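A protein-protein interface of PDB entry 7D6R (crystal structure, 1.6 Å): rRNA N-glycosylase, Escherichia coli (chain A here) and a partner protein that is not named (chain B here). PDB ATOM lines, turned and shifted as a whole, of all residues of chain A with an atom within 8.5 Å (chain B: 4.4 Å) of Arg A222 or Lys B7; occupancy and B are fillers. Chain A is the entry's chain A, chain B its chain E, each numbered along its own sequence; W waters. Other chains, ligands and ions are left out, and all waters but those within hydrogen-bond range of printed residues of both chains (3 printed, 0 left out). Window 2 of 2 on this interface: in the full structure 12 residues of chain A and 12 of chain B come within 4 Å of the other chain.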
ATOM      1  N   PRO A 193      -1.424  26.434   3.596  1.00  0.00           N
ATOM      2  CA  PRO A 193      -1.058  25.074   3.180  1.00  0.00           C
ATOM      3  C   PRO A 193       0.376  24.716   3.523  1.00  0.00           C
ATOM      4  O   PRO A 193       0.642  23.568   3.892  1.00  0.00           O
ATOM      5  CB  PRO A 193      -1.305  25.106   1.662  1.00  0.00           C
ATOM      6  CG  PRO A 193      -2.375  26.121   1.487  1.00  0.00           C
ATOM      7  CD  PRO A 193      -2.063  27.190   2.506  1.00  0.00           C
ATOM      8  N   GLY A 194       1.311  25.665   3.427  1.00  0.00           N
ATOM      9  CA  GLY A 194       2.694  25.355   3.763  1.00  0.00           C
ATOM     10  C   GLY A 194       2.885  25.052   5.240  1.00  0.00           C
ATOM     11  O   GLY A 194       3.642  24.144   5.606  1.00  0.00           O
ATOM     12  N   VAL A 196       0.594  23.727   7.138  1.00  0.00           N
ATOM     13  CA  VAL A 196       0.013  22.401   7.313  1.00  0.00           C
ATOM     14  C   VAL A 196       0.992  21.329   6.841  1.00  0.00           C
ATOM     15  O   VAL A 196       1.226  20.326   7.530  1.00  0.00           O
ATOM     16  CB  VAL A 196      -1.333  22.316   6.570  1.00  0.00           C
ATOM     17  CG1 VAL A 196      -1.839  20.884   6.553  1.00  0.00           C
ATOM     18  CG2 VAL A 196      -2.349  23.269   7.207  1.00  0.00           C
ATOM     19  N   ASP A 197       1.594  21.538   5.664  1.00  0.00           N
ATOM     20  CA  ASP A 197       2.551  20.574   5.128  1.00  0.00           C
ATOM     21  C   ASP A 197       3.732  20.375   6.075  1.00  0.00           C
ATOM     22  O   ASP A 197       4.220  19.250   6.248  1.00  0.00           O
ATOM     23  CB  ASP A 197       3.046  21.033   3.752  1.00  0.00           C
ATOM     24  CG  ASP A 197       2.143  20.584   2.615  1.00  0.00           C
ATOM     25  OD1 ASP A 197       1.321  19.662   2.811  1.00  0.00           O
ATOM     26  OD2 ASP A 197       2.265  21.159   1.513  1.00  0.00           O
ATOM     27  N   LEU A 198       4.215  21.460   6.700  1.00  0.00           N
ATOM     28  CA  LEU A 198       5.277  21.297   7.691  1.00  0.00           C
ATOM     29  C   LEU A 198       4.853  20.323   8.781  1.00  0.00           C
ATOM     30  O   LEU A 198       5.583  19.364   9.112  1.00  0.00           O
ATOM     31  CB  LEU A 198       5.647  22.647   8.312  1.00  0.00           C
ATOM     32  CG  LEU A 198       6.615  23.526   7.544  1.00  0.00           C
ATOM     33  CD1 LEU A 198       6.744  24.835   8.288  1.00  0.00           C
ATOM     34  CD2 LEU A 198       7.974  22.838   7.408  1.00  0.00           C
ATOM     35  N   LEU A 200       2.687  18.017   8.741  1.00  0.00           N
ATOM     36  CA  LEU A 200       2.537  16.647   8.251  1.00  0.00           C
ATOM     37  C   LEU A 200       3.875  15.975   7.947  1.00  0.00           C
ATOM     38  O   LEU A 200       3.925  14.738   7.863  1.00  0.00           O
ATOM     39  CB  LEU A 200       1.651  16.638   7.006  1.00  0.00           C
ATOM     40  CG  LEU A 200       0.246  17.198   7.247  1.00  0.00           C
ATOM     41  CD1 LEU A 200      -0.496  17.383   5.922  1.00  0.00           C
ATOM     42  CD2 LEU A 200      -0.532  16.305   8.202  1.00  0.00           C
ATOM     43  N   ASN A 201       4.945  16.753   7.770  1.00  0.00           N
ATOM     44  CA  ASN A 201       6.265  16.214   7.447  1.00  0.00           C
ATOM     45  C   ASN A 201       7.214  16.213   8.642  1.00  0.00           C
ATOM     46  O   ASN A 201       8.420  16.024   8.461  1.00  0.00           O
ATOM     47  CB  ASN A 201       6.893  17.019   6.305  1.00  0.00           C
ATOM     48  CG  ASN A 201       6.330  16.649   4.950  1.00  0.00           C
ATOM     49  OD1 ASN A 201       6.786  15.697   4.322  1.00  0.00           O
ATOM     50  ND2 ASN A 201       5.334  17.404   4.493  1.00  0.00           N
ATOM     51  N   ARG A 204       9.357  12.964   9.062  1.00  0.00           N
ATOM     52  CA  ARG A 204      10.330  12.827   7.973  1.00  0.00           C
ATOM     53  C   ARG A 204      11.487  13.818   8.116  1.00  0.00           C
ATOM     54  O   ARG A 204      12.673  13.460   7.934  1.00  0.00           O
ATOM     55  CB  ARG A 204       9.616  13.005   6.632  1.00  0.00           C
ATOM     56  CG  ARG A 204       8.570  11.913   6.394  1.00  0.00           C
ATOM     57  CD  ARG A 204       7.628  12.266   5.258  1.00  0.00           C
ATOM     58  NE  ARG A 204       8.279  12.159   3.956  1.00  0.00           N
ATOM     59  CZ  ARG A 204       7.694  12.470   2.802  1.00  0.00           C
ATOM     60  NH1 ARG A 204       6.446  12.928   2.788  1.00  0.00           N
ATOM     61  NH2 ARG A 204       8.358  12.340   1.665  1.00  0.00           N
ATOM     62  N   ILE A 205      11.156  15.073   8.449  1.00  0.00           N
ATOM     63  CA  ILE A 205      12.184  16.081   8.695  1.00  0.00           C
ATOM     64  C   ILE A 205      13.092  15.636   9.829  1.00  0.00           C
ATOM     65  O   ILE A 205      14.321  15.818   9.782  1.00  0.00           O
ATOM     66  CB  ILE A 205      11.520  17.433   9.006  1.00  0.00           C
ATOM     67  CG1 ILE A 205      10.842  18.005   7.760  1.00  0.00           C
ATOM     68  CG2 ILE A 205      12.545  18.448   9.553  1.00  0.00           C
ATOM     69  CD1 ILE A 205       9.861  19.161   8.077  1.00  0.00           C
ATOM     70  N   VAL A 218      18.432  21.080   1.669  1.00  0.00           N
ATOM     71  CA  VAL A 218      17.782  19.889   2.205  1.00  0.00           C
ATOM     72  C   VAL A 218      16.435  19.738   1.516  1.00  0.00           C
ATOM     73  O   VAL A 218      15.701  20.718   1.351  1.00  0.00           O
ATOM     74  CB  VAL A 218      17.599  19.970   3.735  1.00  0.00           C
ATOM     75  CG1 VAL A 218      16.879  18.731   4.230  1.00  0.00           C
ATOM     76  CG2 VAL A 218      18.958  20.124   4.422  1.00  0.00           C
ATOM     77  N   ARG A 219      16.108  18.513   1.091  1.00  0.00           N
ATOM     78  CA  ARG A 219      14.834  18.238   0.434  1.00  0.00           C
ATOM     79  C   ARG A 219      14.170  17.058   1.122  1.00  0.00           C
ATOM     80  O   ARG A 219      14.748  15.969   1.181  1.00  0.00           O
ATOM     81  CB  ARG A 219      15.030  17.945  -1.059  1.00  0.00           C
ATOM     82  CG  ARG A 219      15.547  19.134  -1.869  1.00  0.00           C
ATOM     83  CD  ARG A 219      14.447  20.168  -2.087  1.00  0.00           C
ATOM     84  NE  ARG A 219      13.548  19.744  -3.155  1.00  0.00           N
ATOM     85  CZ  ARG A 219      12.332  19.244  -2.972  1.00  0.00           C
ATOM     86  NH1 ARG A 219      11.821  19.108  -1.750  1.00  0.00           N
ATOM     87  NH2 ARG A 219      11.627  18.869  -4.038  1.00  0.00           N
ATOM     88  N   VAL A 220      12.969  17.275   1.654  1.00  0.00           N
ATOM     89  CA  VAL A 220      12.207  16.219   2.326  1.00  0.00           C
ATOM     90  C   VAL A 220      10.800  16.290   1.757  1.00  0.00           C
ATOM     91  O   VAL A 220      10.014  17.152   2.151  1.00  0.00           O
ATOM     92  CB  VAL A 220      12.191  16.383   3.851  1.00  0.00           C
ATOM     93  CG1 VAL A 220      11.352  15.281   4.489  1.00  0.00           C
ATOM     94  CG2 VAL A 220      13.597  16.381   4.412  1.00  0.00           C
ATOM     95  N   GLY A 221      10.465  15.382   0.841  1.00  0.00           N
ATOM     96  CA  GLY A 221       9.150  15.454   0.227  1.00  0.00           C
ATOM     97  C   GLY A 221       8.859  16.819  -0.367  1.00  0.00           C
ATOM     98  O   GLY A 221       9.616  17.314  -1.208  1.00  0.00           O
ATOM     99  N   ARG A 222       7.770  17.448   0.083  1.00  0.00           N
ATOM    100  CA  ARG A 222       7.362  18.742  -0.453  1.00  0.00           C
ATOM    101  C   ARG A 222       8.129  19.902   0.165  1.00  0.00           C
ATOM    102  O   ARG A 222       7.964  21.039  -0.291  1.00  0.00           O
ATOM    103  CB  ARG A 222       5.858  18.938  -0.244  1.00  0.00           C
ATOM    104  CG  ARG A 222       5.019  17.888  -0.986  1.00  0.00           C
ATOM    105  CD  ARG A 222       3.642  17.681  -0.372  1.00  0.00           C
ATOM    106  NE  ARG A 222       2.773  18.863  -0.374  1.00  0.00           N
ATOM    107  CZ  ARG A 222       2.045  19.276  -1.411  1.00  0.00           C
ATOM    108  NH1 ARG A 222       2.096  18.629  -2.578  1.00  0.00           N
ATOM    109  NH2 ARG A 222       1.254  20.338  -1.290  1.00  0.00           N
ATOM    110  N   ILE A 223       8.980  19.632   1.150  1.00  0.00           N
ATOM    111  CA  ILE A 223       9.673  20.662   1.927  1.00  0.00           C
ATOM    112  C   ILE A 223      11.071  20.887   1.352  1.00  0.00           C
ATOM    113  O   ILE A 223      11.820  19.924   1.114  1.00  0.00           O
ATOM    114  CB  ILE A 223       9.754  20.255   3.409  1.00  0.00           C
ATOM    115  CG1 ILE A 223       8.380  19.821   3.939  1.00  0.00           C
ATOM    116  CG2 ILE A 223      10.359  21.389   4.245  1.00  0.00           C
ATOM    117  CD1 ILE A 223       7.322  20.901   3.882  1.00  0.00           C
ATOM    118  N   SER A 224      11.437  22.162   1.153  1.00  0.00           N
ATOM    119  CA  SER A 224      12.754  22.543   0.649  1.00  0.00           C
ATOM    120  C   SER A 224      13.381  23.577   1.569  1.00  0.00           C
ATOM    121  O   SER A 224      12.723  24.555   1.935  1.00  0.00           O
ATOM    122  CB  SER A 224      12.670  23.139  -0.760  1.00  0.00           C
ATOM    123  OG  SER A 224      12.080  22.243  -1.678  1.00  0.00           O
ATOM    124  N   PHE A 225      14.654  23.372   1.913  1.00  0.00           N
ATOM    125  CA  PHE A 225      15.460  24.368   2.626  1.00  0.00           C
ATOM    126  C   PHE A 225      16.694  24.662   1.790  1.00  0.00           C
ATOM    127  O   PHE A 225      17.449  23.747   1.453  1.00  0.00           O
ATOM    128  CB  PHE A 225      15.889  23.867   4.006  1.00  0.00           C
ATOM    129  CG  PHE A 225      14.759  23.476   4.900  1.00  0.00           C
ATOM    130  CD1 PHE A 225      13.724  24.353   5.169  1.00  0.00           C
ATOM    131  CD2 PHE A 225      14.739  22.228   5.492  1.00  0.00           C
ATOM    132  CE1 PHE A 225      12.683  23.977   6.013  1.00  0.00           C
ATOM    133  CE2 PHE A 225      13.698  21.851   6.332  1.00  0.00           C
ATOM    134  CZ  PHE A 225      12.674  22.728   6.589  1.00  0.00           C
ATOM    135  N   TRP A 276      18.910  14.847   0.332  1.00  0.00           N
ATOM    136  CA  TRP A 276      17.555  14.390   0.058  1.00  0.00           C
ATOM    137  C   TRP A 276      17.152  13.297   1.034  1.00  0.00           C
ATOM    138  O   TRP A 276      17.938  12.395   1.333  1.00  0.00           O
ATOM    139  CB  TRP A 276      17.446  13.806  -1.358  1.00  0.00           C
ATOM    140  CG  TRP A 276      17.452  14.811  -2.478  1.00  0.00           C
ATOM    141  CD1 TRP A 276      18.541  15.438  -3.014  1.00  0.00           C
ATOM    142  CD2 TRP A 276      16.314  15.310  -3.178  1.00  0.00           C
ATOM    143  NE1 TRP A 276      18.150  16.287  -4.014  1.00  0.00           N
ATOM    144  CE2 TRP A 276      16.787  16.226  -4.138  1.00  0.00           C
ATOM    145  CE3 TRP A 276      14.939  15.060  -3.100  1.00  0.00           C
ATOM    146  CZ2 TRP A 276      15.934  16.901  -5.003  1.00  0.00           C
ATOM    147  CZ3 TRP A 276      14.094  15.733  -3.957  1.00  0.00           C
ATOM    148  CH2 TRP A 276      14.593  16.645  -4.898  1.00  0.00           C
ATOM    149  N   GLU A 277      15.909  13.352   1.492  1.00  0.00           N
ATOM    150  CA  GLU A 277      15.295  12.153   2.048  1.00  0.00           C
ATOM    151  C   GLU A 277      15.363  11.052   1.004  1.00  0.00           C
ATOM    152  O   GLU A 277      14.910  11.250  -0.121  1.00  0.00           O
ATOM    153  CB  GLU A 277      13.848  12.446   2.417  1.00  0.00           C
ATOM    154  CG  GLU A 277      13.164  11.264   3.095  1.00  0.00           C
ATOM    155  CD  GLU A 277      11.665  11.380   3.092  1.00  0.00           C
ATOM    156  OE1 GLU A 277      11.087  11.466   2.003  1.00  0.00           O
ATOM    157  OE2 GLU A 277      11.070  11.379   4.183  1.00  0.00           O
ATOM    158  N   THR A 280      12.107  10.135  -0.858  1.00  0.00           N
ATOM    159  CA  THR A 280      11.607  11.058  -1.875  1.00  0.00           C
ATOM    160  C   THR A 280      12.256  10.781  -3.229  1.00  0.00           C
ATOM    161  O   THR A 280      11.574  10.654  -4.265  1.00  0.00           O
ATOM    162  CB  THR A 280      11.877  12.500  -1.424  1.00  0.00           C
ATOM    163  OG1 THR A 280      11.162  12.759  -0.208  1.00  0.00           O
ATOM    164  CG2 THR A 280      11.447  13.504  -2.485  1.00  0.00           C
ATOM    165  N   GLY B   6       0.047  26.417  -8.470  1.00  0.00           N
ATOM    166  CA  GLY B   6       0.254  26.071  -7.081  1.00  0.00           C
ATOM    167  C   GLY B   6       0.771  24.656  -6.957  1.00  0.00           C
ATOM    168  O   GLY B   6       1.012  23.969  -7.951  1.00  0.00           O
ATOM    169  N   LYS B   7       0.970  24.248  -5.705  1.00  0.00           N
ATOM    170  CA  LYS B   7       1.321  22.861  -5.435  1.00  0.00           C
ATOM    171  C   LYS B   7       0.086  21.974  -5.597  1.00  0.00           C
ATOM    172  O   LYS B   7      -1.055  22.434  -5.536  1.00  0.00           O
ATOM    173  CB  LYS B   7       1.907  22.704  -4.031  1.00  0.00           C
ATOM    174  CG  LYS B   7       3.251  23.415  -3.822  1.00  0.00           C
ATOM    175  CD  LYS B   7       3.849  23.060  -2.462  1.00  0.00           C
ATOM    176  CE  LYS B   7       5.219  23.687  -2.252  1.00  0.00           C
ATOM    177  NZ  LYS B   7       5.895  23.053  -1.078  1.00  0.00           N
ATOM    178  N   ILE B   8       0.321  20.683  -5.806  1.00  0.00           N
ATOM    179  CA  ILE B   8      -0.782  19.741  -5.986  1.00  0.00           C
ATOM    180  C   ILE B   8      -1.287  19.300  -4.616  1.00  0.00           C
ATOM    181  O   ILE B   8      -0.537  18.725  -3.823  1.00  0.00           O
ATOM    182  CB  ILE B   8      -0.349  18.535  -6.832  1.00  0.00           C
ATOM    183  CG1 ILE B   8      -0.070  18.963  -8.274  1.00  0.00           C
ATOM    184  CG2 ILE B   8      -1.414  17.424  -6.776  1.00  0.00           C
ATOM    185  CD1 ILE B   8       0.691  17.912  -9.063  1.00  0.00           C
ATOM    186  N   GLU B   9      -2.573  19.548  -4.345  1.00  0.00           N
ATOM    187  CA  GLU B   9      -3.149  19.226  -3.041  1.00  0.00           C
ATOM    188  C   GLU B   9      -3.451  17.736  -2.903  1.00  0.00           C
ATOM    189  O   GLU B   9      -3.177  17.136  -1.861  1.00  0.00           O
ATOM    190  CB  GLU B   9      -4.416  20.053  -2.818  1.00  0.00           C
ATOM    191  CG  GLU B   9      -5.161  19.703  -1.545  1.00  0.00           C
ATOM    192  CD  GLU B   9      -6.387  20.570  -1.308  1.00  0.00           C
ATOM    193  OE1 GLU B   9      -7.185  20.226  -0.408  1.00  0.00           O
ATOM    194  OE2 GLU B   9      -6.547  21.591  -2.010  1.00  0.00           O
ATOM    195  N   LYS B  22      -5.829  18.407  -7.865  1.00  0.00           N
ATOM    196  CA  LYS B  22      -6.394  19.625  -7.294  1.00  0.00           C
ATOM    197  C   LYS B  22      -5.282  20.647  -7.116  1.00  0.00           C
ATOM    198  O   LYS B  22      -4.292  20.377  -6.425  1.00  0.00           O
ATOM    199  CB  LYS B  22      -7.093  19.356  -5.964  1.00  0.00           C
ATOM    200  CG  LYS B  22      -7.817  20.603  -5.452  1.00  0.00           C
ATOM    201  CD  LYS B  22      -8.867  20.263  -4.422  1.00  0.00           C
ATOM    202  CE  LYS B  22      -9.584  21.520  -3.939  1.00  0.00           C
ATOM    203  NZ  LYS B  22     -10.397  21.247  -2.725  1.00  0.00           N
ATOM    204  N   VAL B  23      -5.452  21.814  -7.733  1.00  0.00           N
ATOM    205  CA  VAL B  23      -4.454  22.879  -7.733  1.00  0.00           C
ATOM    206  C   VAL B  23      -5.174  24.185  -7.428  1.00  0.00           C
ATOM    207  O   VAL B  23      -6.109  24.557  -8.143  1.00  0.00           O
ATOM    208  CB  VAL B  23      -3.710  22.971  -9.075  1.00  0.00           C
ATOM    209  CG1 VAL B  23      -2.650  24.069  -9.023  1.00  0.00           C
ATOM    210  CG2 VAL B  23      -3.085  21.616  -9.437  1.00  0.00           C
ATOM    211  N   GLN B  43       3.670  16.237  -7.241  1.00  0.00           N
ATOM    212  CA  GLN B  43       2.957  16.284  -5.974  1.00  0.00           C
ATOM    213  C   GLN B  43       3.888  15.959  -4.816  1.00  0.00           C
ATOM    214  O   GLN B  43       3.927  16.688  -3.814  1.00  0.00           O
ATOM    215  CB  GLN B  43       1.765  15.318  -6.005  1.00  0.00           C
ATOM    216  CG  GLN B  43       0.964  15.302  -4.697  1.00  0.00           C
ATOM    217  CD  GLN B  43      -0.171  14.281  -4.742  1.00  0.00           C
ATOM    218  OE1 GLN B  43      -0.478  13.730  -5.801  1.00  0.00           O
ATOM    219  NE2 GLN B  43      -0.800  14.037  -3.595  1.00  0.00           N
ATOM    220  N   LEU B  44       4.689  14.895  -4.948  1.00  0.00           N
ATOM    221  CA  LEU B  44       5.382  14.423  -3.759  1.00  0.00           C
ATOM    222  C   LEU B  44       6.653  15.210  -3.484  1.00  0.00           C
ATOM    223  O   LEU B  44       7.184  15.131  -2.373  1.00  0.00           O
ATOM    224  CB  LEU B  44       5.666  12.916  -3.869  1.00  0.00           C
ATOM    225  CG  LEU B  44       6.638  12.402  -4.931  1.00  0.00           C
ATOM    226  CD1 LEU B  44       8.050  12.337  -4.385  1.00  0.00           C
ATOM    227  CD2 LEU B  44       6.195  11.009  -5.391  1.00  0.00           C
ATOM    228  N   THR B  45       7.137  15.972  -4.471  1.00  0.00           N
ATOM    229  CA  THR B  45       8.302  16.835  -4.311  1.00  0.00           C
ATOM    230  C   THR B  45       7.932  18.294  -4.110  1.00  0.00           C
ATOM    231  O   THR B  45       8.836  19.127  -3.950  1.00  0.00           O
ATOM    232  CB  THR B  45       9.231  16.746  -5.530  1.00  0.00           C
ATOM    233  OG1 THR B  45       8.528  17.176  -6.702  1.00  0.00           O
ATOM    234  CG2 THR B  45       9.774  15.329  -5.733  1.00  0.00           C
ATOM    235  N   GLY B  46       6.645  18.628  -4.142  1.00  0.00           N
ATOM    236  CA  GLY B  46       6.250  20.002  -3.891  1.00  0.00           C
ATOM    237  C   GLY B  46       6.555  20.972  -5.013  1.00  0.00           C
ATOM    238  O   GLY B  46       6.770  22.161  -4.754  1.00  0.00           O
ATOM    239  N   MET B  47       6.575  20.501  -6.254  1.00  0.00           N
ATOM    240  CA  MET B  47       6.739  21.409  -7.377  1.00  0.00           C
ATOM    241  C   MET B  47       5.524  22.322  -7.510  1.00  0.00           C
ATOM    242  O   MET B  47       4.399  21.961  -7.160  1.00  0.00           O
ATOM    243  CB  MET B  47       6.938  20.621  -8.678  1.00  0.00           C
ATOM    244  CG  MET B  47       8.248  19.856  -8.758  1.00  0.00           C
ATOM    245  SD  MET B  47       8.455  19.071 -10.389  1.00  0.00           S
ATOM    246  CE  MET B  47       9.540  20.246 -11.201  1.00  0.00           C
HETATM  247  O   HOH W   1      -1.150  22.009  -2.245  1.00  0.00           O
HETATM  248  O   HOH W   2       4.234  22.867   1.235  1.00  0.00           O
HETATM  249  O   HOH W   3       6.397  13.439  -0.290  1.00  0.00           O
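The guanidinium group (NH2) of Arg A219 is in hydrogen-bond range of the backbone carbonyl oxygen (O) of Thr B45 (2.8 Å). The guanidinium group of Arg A222 is in hydrogen-bond range of the backbone carbonyl oxygen of Gln B43 (2.9 Å). O of Arg A222 is in hydrogen-bond range of NZ of Lys B7. The backbone carbonyl oxygen (O) of Thr B45 sits close to the backbone carbonyl oxygen (O) of Gly A221 (3.4 Å). The backbone carbonyl oxygen (O) of Gly A221 sits close to the backbone carbonyl oxygen (O) of Leu B44 (3.5 Å). O of Leu B44 sits at hydrogen-bond distance from N of Arg A222, 3.4 Å away. NH1 of Arg A222 sits at hydrogen-bond distance from O of Ile B8, at 2.9 Å.
The side-chain hydroxyl (OG1) of Thr A280 sits at hydrogen-bond distance from the backbone NH (N) of Gly A221 (2.9 Å). The side-chain hydroxyl of Thr A280 sits at hydrogen-bond distance from the guanidinium group of Arg A204, at 3.4 Å. The backbone NH (N) of Glu A277 sits at hydrogen-bond distance from the backbone carbonyl oxygen (O) of Arg A219 (2.9 Å). The guanidinium group of Arg A219 lies within hydrogen-bond range of the backbone carbonyl oxygen of Gly A221 (2.9 Å). NE of Arg A222 lies within salt-bridge range of OD2 of Asp A197. The guanidinium group (NH1) of Arg A219 sits at hydrogen-bond distance from the backbone carbonyl oxygen (O) of Ile A223.
Thr B45 touches Arg A222 (C to CA, 3.7 Å). Gly B46 touches Arg A222. Thr A280 touches Leu B44 (O to CD1, 3.9 Å).
Of the printed residues of chain B, Arg A219 touches Thr B45 (2.8 Å). Printed residues of chain B within 4 Å of Gly A221: Leu B44 (3.1 Å) and Thr B45 (3.4 Å). Arg A222 touches just these residues of chain B: Lys B7, Ile B8, Gln B43, Leu B44, Thr B45 and Gly B46. No residue of chain A comes within 4 Å of Gly B6. Printed residues of chain A within 4 Å of Lys B7: Arg A222 (3.0 Å). Printed residues of chain A within 4 Å of Ile B8: Arg A222. Of the printed residues of chain A, Gln B43 touches Arg A222. Printed residues of chain A within 4 Å of Leu B44: Gly A221, Arg A222 and Thr A280. Of chain A, only Arg A222 comes within 4 Å of Gly B46. The nearest printed residue of chain B that does not touch Arg A222 is Glu B9 (4.9 Å).
Hydrophobic or aromatic side chains of chain B that line the printed part of chain A: Leu B44. Of the 20 printed residues of chain A, 4 touch a printed residue of chain B. Among the printed residues, no Asp or Glu carboxylate lies within 4 Å of a Lys or Arg side-chain nitrogen of the other chain.
Water W2 lies within hydrogen-bond range of the side-chain carboxylate (OD2) of Asp A197 (2.6 Å) and the side-chain amino group (NZ) of Lys B7 (2.9 Å). Water W3 lies within hydrogen-bond range of the backbone carbonyl oxygen (O) of Leu B44 and the guanidinium group (NH2) of Arg A204. Water W1 bridges NH2 of Arg A222 (3.1 Å) and O of Lys B7 (3.3 Å).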
